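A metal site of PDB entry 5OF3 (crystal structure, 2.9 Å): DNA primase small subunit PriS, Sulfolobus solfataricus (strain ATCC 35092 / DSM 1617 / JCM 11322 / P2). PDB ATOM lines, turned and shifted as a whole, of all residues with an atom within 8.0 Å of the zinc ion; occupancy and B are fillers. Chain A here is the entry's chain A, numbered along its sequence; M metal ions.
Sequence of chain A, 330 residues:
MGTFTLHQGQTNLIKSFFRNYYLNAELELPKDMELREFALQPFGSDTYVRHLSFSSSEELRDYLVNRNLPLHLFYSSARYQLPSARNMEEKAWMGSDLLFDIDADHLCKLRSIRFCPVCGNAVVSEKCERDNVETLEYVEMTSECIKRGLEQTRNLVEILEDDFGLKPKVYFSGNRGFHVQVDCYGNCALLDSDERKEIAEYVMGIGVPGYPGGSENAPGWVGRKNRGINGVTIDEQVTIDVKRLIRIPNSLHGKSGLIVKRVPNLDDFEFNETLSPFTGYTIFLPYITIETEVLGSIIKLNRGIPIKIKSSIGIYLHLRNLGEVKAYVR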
ATOM      1  N   PHE A 115      -0.120 -30.056  -7.518  1.00  0.00           N
ATOM      2  CA  PHE A 115      -0.656 -28.841  -8.103  1.00  0.00           C
ATOM      3  C   PHE A 115      -2.159 -28.969  -8.261  1.00  0.00           C
ATOM      4  O   PHE A 115      -2.733 -30.057  -8.155  1.00  0.00           O
ATOM      5  CB  PHE A 115       0.014 -28.535  -9.441  1.00  0.00           C
ATOM      6  CG  PHE A 115      -0.169 -29.619 -10.474  1.00  0.00           C
ATOM      7  CD1 PHE A 115      -1.323 -29.658 -11.252  1.00  0.00           C
ATOM      8  CD2 PHE A 115       0.805 -30.582 -10.664  1.00  0.00           C
ATOM      9  CE1 PHE A 115      -1.491 -30.655 -12.202  1.00  0.00           C
ATOM     10  CE2 PHE A 115       0.637 -31.572 -11.620  1.00  0.00           C
ATOM     11  CZ  PHE A 115      -0.511 -31.612 -12.386  1.00  0.00           C
ATOM     12  N   CYS A 116      -2.797 -27.832  -8.566  1.00  0.00           N
ATOM     13  CA  CYS A 116      -4.213 -27.787  -8.868  1.00  0.00           C
ATOM     14  C   CYS A 116      -4.407 -27.743 -10.366  1.00  0.00           C
ATOM     15  O   CYS A 116      -3.851 -26.849 -11.025  1.00  0.00           O
ATOM     16  CB  CYS A 116      -4.856 -26.571  -8.214  1.00  0.00           C
ATOM     17  SG  CYS A 116      -6.485 -26.144  -8.857  1.00  0.00           S
ATOM     18  N   PRO A 117      -5.168 -28.669 -10.957  1.00  0.00           N
ATOM     19  CA  PRO A 117      -5.316 -28.699 -12.418  1.00  0.00           C
ATOM     20  C   PRO A 117      -6.173 -27.569 -12.982  1.00  0.00           C
ATOM     21  O   PRO A 117      -6.322 -27.498 -14.205  1.00  0.00           O
ATOM     22  CB  PRO A 117      -5.975 -30.066 -12.677  1.00  0.00           C
ATOM     23  CG  PRO A 117      -6.719 -30.346 -11.421  1.00  0.00           C
ATOM     24  CD  PRO A 117      -5.890 -29.784 -10.308  1.00  0.00           C
ATOM     25  N   VAL A 118      -6.734 -26.697 -12.152  1.00  0.00           N
ATOM     26  CA  VAL A 118      -7.619 -25.637 -12.615  1.00  0.00           C
ATOM     27  C   VAL A 118      -6.903 -24.291 -12.645  1.00  0.00           C
ATOM     28  O   VAL A 118      -6.996 -23.566 -13.639  1.00  0.00           O
ATOM     29  CB  VAL A 118      -8.891 -25.576 -11.734  1.00  0.00           C
ATOM     30  CG1 VAL A 118      -9.840 -24.521 -12.254  1.00  0.00           C
ATOM     31  CG2 VAL A 118      -9.559 -26.940 -11.710  1.00  0.00           C
ATOM     32  N   CYS A 119      -6.201 -23.936 -11.573  1.00  0.00           N
ATOM     33  CA  CYS A 119      -5.450 -22.700 -11.532  1.00  0.00           C
ATOM     34  C   CYS A 119      -3.982 -22.868 -11.871  1.00  0.00           C
ATOM     35  O   CYS A 119      -3.306 -21.885 -12.199  1.00  0.00           O
ATOM     36  CB  CYS A 119      -5.577 -22.043 -10.155  1.00  0.00           C
ATOM     37  SG  CYS A 119      -4.779 -22.958  -8.817  1.00  0.00           S
ATOM     38  N   GLY A 120      -3.463 -24.092 -11.798  1.00  0.00           N
ATOM     39  CA  GLY A 120      -2.115 -24.369 -12.222  1.00  0.00           C
ATOM     40  C   GLY A 120      -1.025 -23.998 -11.241  1.00  0.00           C
ATOM     41  O   GLY A 120       0.121 -23.784 -11.649  1.00  0.00           O
ATOM     42  N   ASN A 121      -1.341 -23.938  -9.946  1.00  0.00           N
ATOM     43  CA  ASN A 121      -0.391 -23.513  -8.933  1.00  0.00           C
ATOM     44  C   ASN A 121       0.061 -24.718  -8.109  1.00  0.00           C
ATOM     45  O   ASN A 121      -0.699 -25.669  -7.913  1.00  0.00           O
ATOM     46  CB  ASN A 121      -1.000 -22.470  -8.002  1.00  0.00           C
ATOM     47  CG  ASN A 121      -1.238 -21.148  -8.697  1.00  0.00           C
ATOM     48  OD1 ASN A 121      -0.417 -20.689  -9.489  1.00  0.00           O
ATOM     49  ND2 ASN A 121      -2.371 -20.517  -8.402  1.00  0.00           N
ATOM     50  N   ALA A 122       1.306 -24.669  -7.649  1.00  0.00           N
ATOM     51  CA  ALA A 122       1.780 -25.666  -6.707  1.00  0.00           C
ATOM     52  C   ALA A 122       1.017 -25.564  -5.398  1.00  0.00           C
ATOM     53  O   ALA A 122       0.939 -24.483  -4.800  1.00  0.00           O
ATOM     54  CB  ALA A 122       3.286 -25.501  -6.471  1.00  0.00           C
ATOM     55  N   VAL A 123       0.433 -26.681  -4.956  1.00  0.00           N
ATOM     56  CA  VAL A 123      -0.423 -26.717  -3.776  1.00  0.00           C
ATOM     57  C   VAL A 123      -0.069 -27.964  -2.974  1.00  0.00           C
ATOM     58  O   VAL A 123      -0.067 -29.071  -3.509  1.00  0.00           O
ATOM     59  CB  VAL A 123      -1.914 -26.720  -4.149  1.00  0.00           C
ATOM     60  CG1 VAL A 123      -2.767 -26.862  -2.891  1.00  0.00           C
ATOM     61  CG2 VAL A 123      -2.289 -25.444  -4.894  1.00  0.00           C
ATOM     62  N   LYS A 127      -6.841 -30.566  -1.569  1.00  0.00           N
ATOM     63  CA  LYS A 127      -7.770 -29.766  -2.352  1.00  0.00           C
ATOM     64  C   LYS A 127      -7.191 -28.374  -2.567  1.00  0.00           C
ATOM     65  O   LYS A 127      -6.234 -27.958  -1.913  1.00  0.00           O
ATOM     66  CB  LYS A 127      -9.140 -29.659  -1.673  1.00  0.00           C
ATOM     67  CG  LYS A 127      -9.903 -30.967  -1.573  1.00  0.00           C
ATOM     68  CD  LYS A 127     -11.400 -30.720  -1.673  1.00  0.00           C
ATOM     69  CE  LYS A 127     -12.181 -32.021  -1.720  1.00  0.00           C
ATOM     70  NZ  LYS A 127     -13.399 -31.909  -2.570  1.00  0.00           N
ATOM     71  N   CYS A 128      -7.782 -27.659  -3.512  1.00  0.00           N
ATOM     72  CA  CYS A 128      -7.465 -26.256  -3.743  1.00  0.00           C
ATOM     73  C   CYS A 128      -8.608 -25.422  -3.192  1.00  0.00           C
ATOM     74  O   CYS A 128      -9.781 -25.729  -3.420  1.00  0.00           O
ATOM     75  CB  CYS A 128      -7.270 -25.983  -5.237  1.00  0.00           C
ATOM     76  SG  CYS A 128      -6.824 -24.275  -5.639  1.00  0.00           S
ATOM     77  N   GLU A 129      -8.264 -24.366  -2.448  1.00  0.00           N
ATOM     78  CA  GLU A 129      -9.285 -23.563  -1.783  1.00  0.00           C
ATOM     79  C   GLU A 129     -10.189 -22.878  -2.793  1.00  0.00           C
ATOM     80  O   GLU A 129     -11.419 -22.966  -2.705  1.00  0.00           O
ATOM     81  CB  GLU A 129      -8.632 -22.547  -0.845  1.00  0.00           C
ATOM     82  CG  GLU A 129      -8.400 -23.076   0.555  1.00  0.00           C
ATOM     83  CD  GLU A 129      -9.640 -22.981   1.424  1.00  0.00           C
ATOM     84  OE1 GLU A 129     -10.391 -21.999   1.268  1.00  0.00           O
ATOM     85  OE2 GLU A 129      -9.861 -23.888   2.259  1.00  0.00           O
ATOM     86  N   ARG A 130      -9.597 -22.174  -3.765  1.00  0.00           N
ATOM     87  CA  ARG A 130     -10.354 -21.435  -4.759  1.00  0.00           C
ATOM     88  C   ARG A 130     -11.297 -22.350  -5.525  1.00  0.00           C
ATOM     89  O   ARG A 130     -12.524 -22.302  -5.345  1.00  0.00           O
ATOM     90  CB  ARG A 130      -9.429 -20.764  -5.770  1.00  0.00           C
ATOM     91  CG  ARG A 130      -8.392 -19.820  -5.207  1.00  0.00           C
ATOM     92  CD  ARG A 130      -7.671 -19.160  -6.369  1.00  0.00           C
ATOM     93  NE  ARG A 130      -6.269 -18.906  -6.083  1.00  0.00           N
ATOM     94  CZ  ARG A 130      -5.387 -18.495  -6.982  1.00  0.00           C
ATOM     95  NH1 ARG A 130      -4.121 -18.285  -6.646  1.00  0.00           N
ATOM     96  NH2 ARG A 130      -5.764 -18.284  -8.235  1.00  0.00           N
ATOM     97  N   ASP A 131     -10.723 -23.199  -6.375  1.00  0.00           N
ATOM     98  CA  ASP A 131     -11.472 -23.952  -7.372  1.00  0.00           C
ATOM     99  C   ASP A 131     -12.235 -25.124  -6.761  1.00  0.00           C
ATOM    100  O   ASP A 131     -13.109 -25.678  -7.444  1.00  0.00           O
ATOM    101  CB  ASP A 131     -10.516 -24.449  -8.448  1.00  0.00           C
ATOM    102  CG  ASP A 131      -9.514 -23.390  -8.876  1.00  0.00           C
ATOM    103  OD1 ASP A 131      -9.931 -22.225  -9.083  1.00  0.00           O
ATOM    104  OD2 ASP A 131      -8.309 -23.704  -8.991  1.00  0.00           O
ATOM    105  N   ASN A 132     -11.949 -25.491  -5.515  1.00  0.00           N
ATOM    106  CA  ASN A 132     -12.589 -26.626  -4.849  1.00  0.00           C
ATOM    107  C   ASN A 132     -12.442 -27.893  -5.690  1.00  0.00           C
ATOM    108  O   ASN A 132     -13.402 -28.635  -5.935  1.00  0.00           O
ATOM    109  CB  ASN A 132     -14.056 -26.333  -4.542  1.00  0.00           C
ATOM    110  CG  ASN A 132     -14.676 -27.349  -3.607  1.00  0.00           C
ATOM    111  OD1 ASN A 132     -14.022 -27.848  -2.693  1.00  0.00           O
ATOM    112  ND2 ASN A 132     -15.940 -27.670  -3.842  1.00  0.00           N
ATOM    113  N   VAL A 133     -11.217 -28.137  -6.157  1.00  0.00           N
ATOM    114  CA  VAL A 133     -10.876 -29.323  -6.932  1.00  0.00           C
ATOM    115  C   VAL A 133      -9.715 -30.022  -6.245  1.00  0.00           C
ATOM    116  O   VAL A 133      -8.839 -29.380  -5.659  1.00  0.00           O
ATOM    117  CB  VAL A 133     -10.527 -28.967  -8.397  1.00  0.00           C
ATOM    118  CG1 VAL A 133     -10.374 -30.228  -9.232  1.00  0.00           C
ATOM    119  CG2 VAL A 133     -11.596 -28.066  -8.989  1.00  0.00           C
ATOM    120  N   GLU A 134      -9.717 -31.344  -6.319  1.00  0.00           N
ATOM    121  CA  GLU A 134      -8.630 -32.135  -5.759  1.00  0.00           C
ATOM    122  C   GLU A 134      -7.332 -31.892  -6.526  1.00  0.00           C
ATOM    123  O   GLU A 134      -7.331 -31.639  -7.735  1.00  0.00           O
ATOM    124  CB  GLU A 134      -8.983 -33.619  -5.788  1.00  0.00           C
ATOM    125  CG  GLU A 134     -10.091 -34.001  -4.819  1.00  0.00           C
ATOM    126  CD  GLU A 134     -10.234 -35.497  -4.662  1.00  0.00           C
ATOM    127  OE1 GLU A 134      -9.351 -36.245  -5.140  1.00  0.00           O
ATOM    128  OE2 GLU A 134     -11.235 -35.941  -4.068  1.00  0.00           O
ATOM    129  N   THR A 135      -6.206 -31.962  -5.811  1.00  0.00           N
ATOM    130  CA  THR A 135      -4.901 -31.733  -6.397  1.00  0.00           C
ATOM    131  C   THR A 135      -4.331 -33.023  -6.991  1.00  0.00           C
ATOM    132  O   THR A 135      -4.475 -34.098  -6.424  1.00  0.00           O
ATOM    133  CB  THR A 135      -3.930 -31.177  -5.354  1.00  0.00           C
ATOM    134  OG1 THR A 135      -3.829 -32.090  -4.251  1.00  0.00           O
ATOM    135  CG2 THR A 135      -4.399 -29.821  -4.854  1.00  0.00           C
ATOM    136  N   ARG A 303       0.905 -23.955 -19.827  1.00  0.00           N
ATOM    137  CA  ARG A 303      -0.433 -24.108 -19.277  1.00  0.00           C
ATOM    138  C   ARG A 303      -1.486 -23.576 -20.245  1.00  0.00           C
ATOM    139  O   ARG A 303      -1.369 -22.464 -20.775  1.00  0.00           O
ATOM    140  CB  ARG A 303      -0.528 -23.367 -17.932  1.00  0.00           C
ATOM    141  CG  ARG A 303      -1.943 -23.266 -17.396  1.00  0.00           C
ATOM    142  CD  ARG A 303      -1.984 -22.410 -16.138  1.00  0.00           C
ATOM    143  NE  ARG A 303      -3.229 -22.607 -15.399  1.00  0.00           N
ATOM    144  CZ  ARG A 303      -4.285 -21.810 -15.492  1.00  0.00           C
ATOM    145  NH1 ARG A 303      -4.259 -20.754 -16.295  1.00  0.00           N
ATOM    146  NH2 ARG A 303      -5.377 -22.065 -14.778  1.00  0.00           N
HETATM  147 ZN    ZN M   1      -6.633 -23.979  -7.950  1.00  0.00          ZN
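O of Asn 121 sits at hydrogen-bond distance from N of Cys 116 (3.1 Å). The side-chain sulfur (SG) of Cys 119 sits close to the side-chain amide nitrogen (ND2) of Asn 121 (3.5 Å). SG of Cys 116 sits close to N of Val 118. The guanidinium group of Arg 303 lies within hydrogen-bond range of the backbone carbonyl oxygen of Cys 119. The backbone NH (N) of Cys 128 is in hydrogen-bond range of the backbone carbonyl oxygen (O) of Val 133, at 2.9 Å.
The zinc ion is bound by OD2 of Asp 131 (2.0 Å), SG of Cys 119 (2.3 Å), SG of Cys 128 (2.3 Å) and SG of Cys 116 (2.4 Å).
Four residues have an atom within 4 Å of the zinc ion: Cys 116, Cys 119, Cys 128 and Asp 131.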
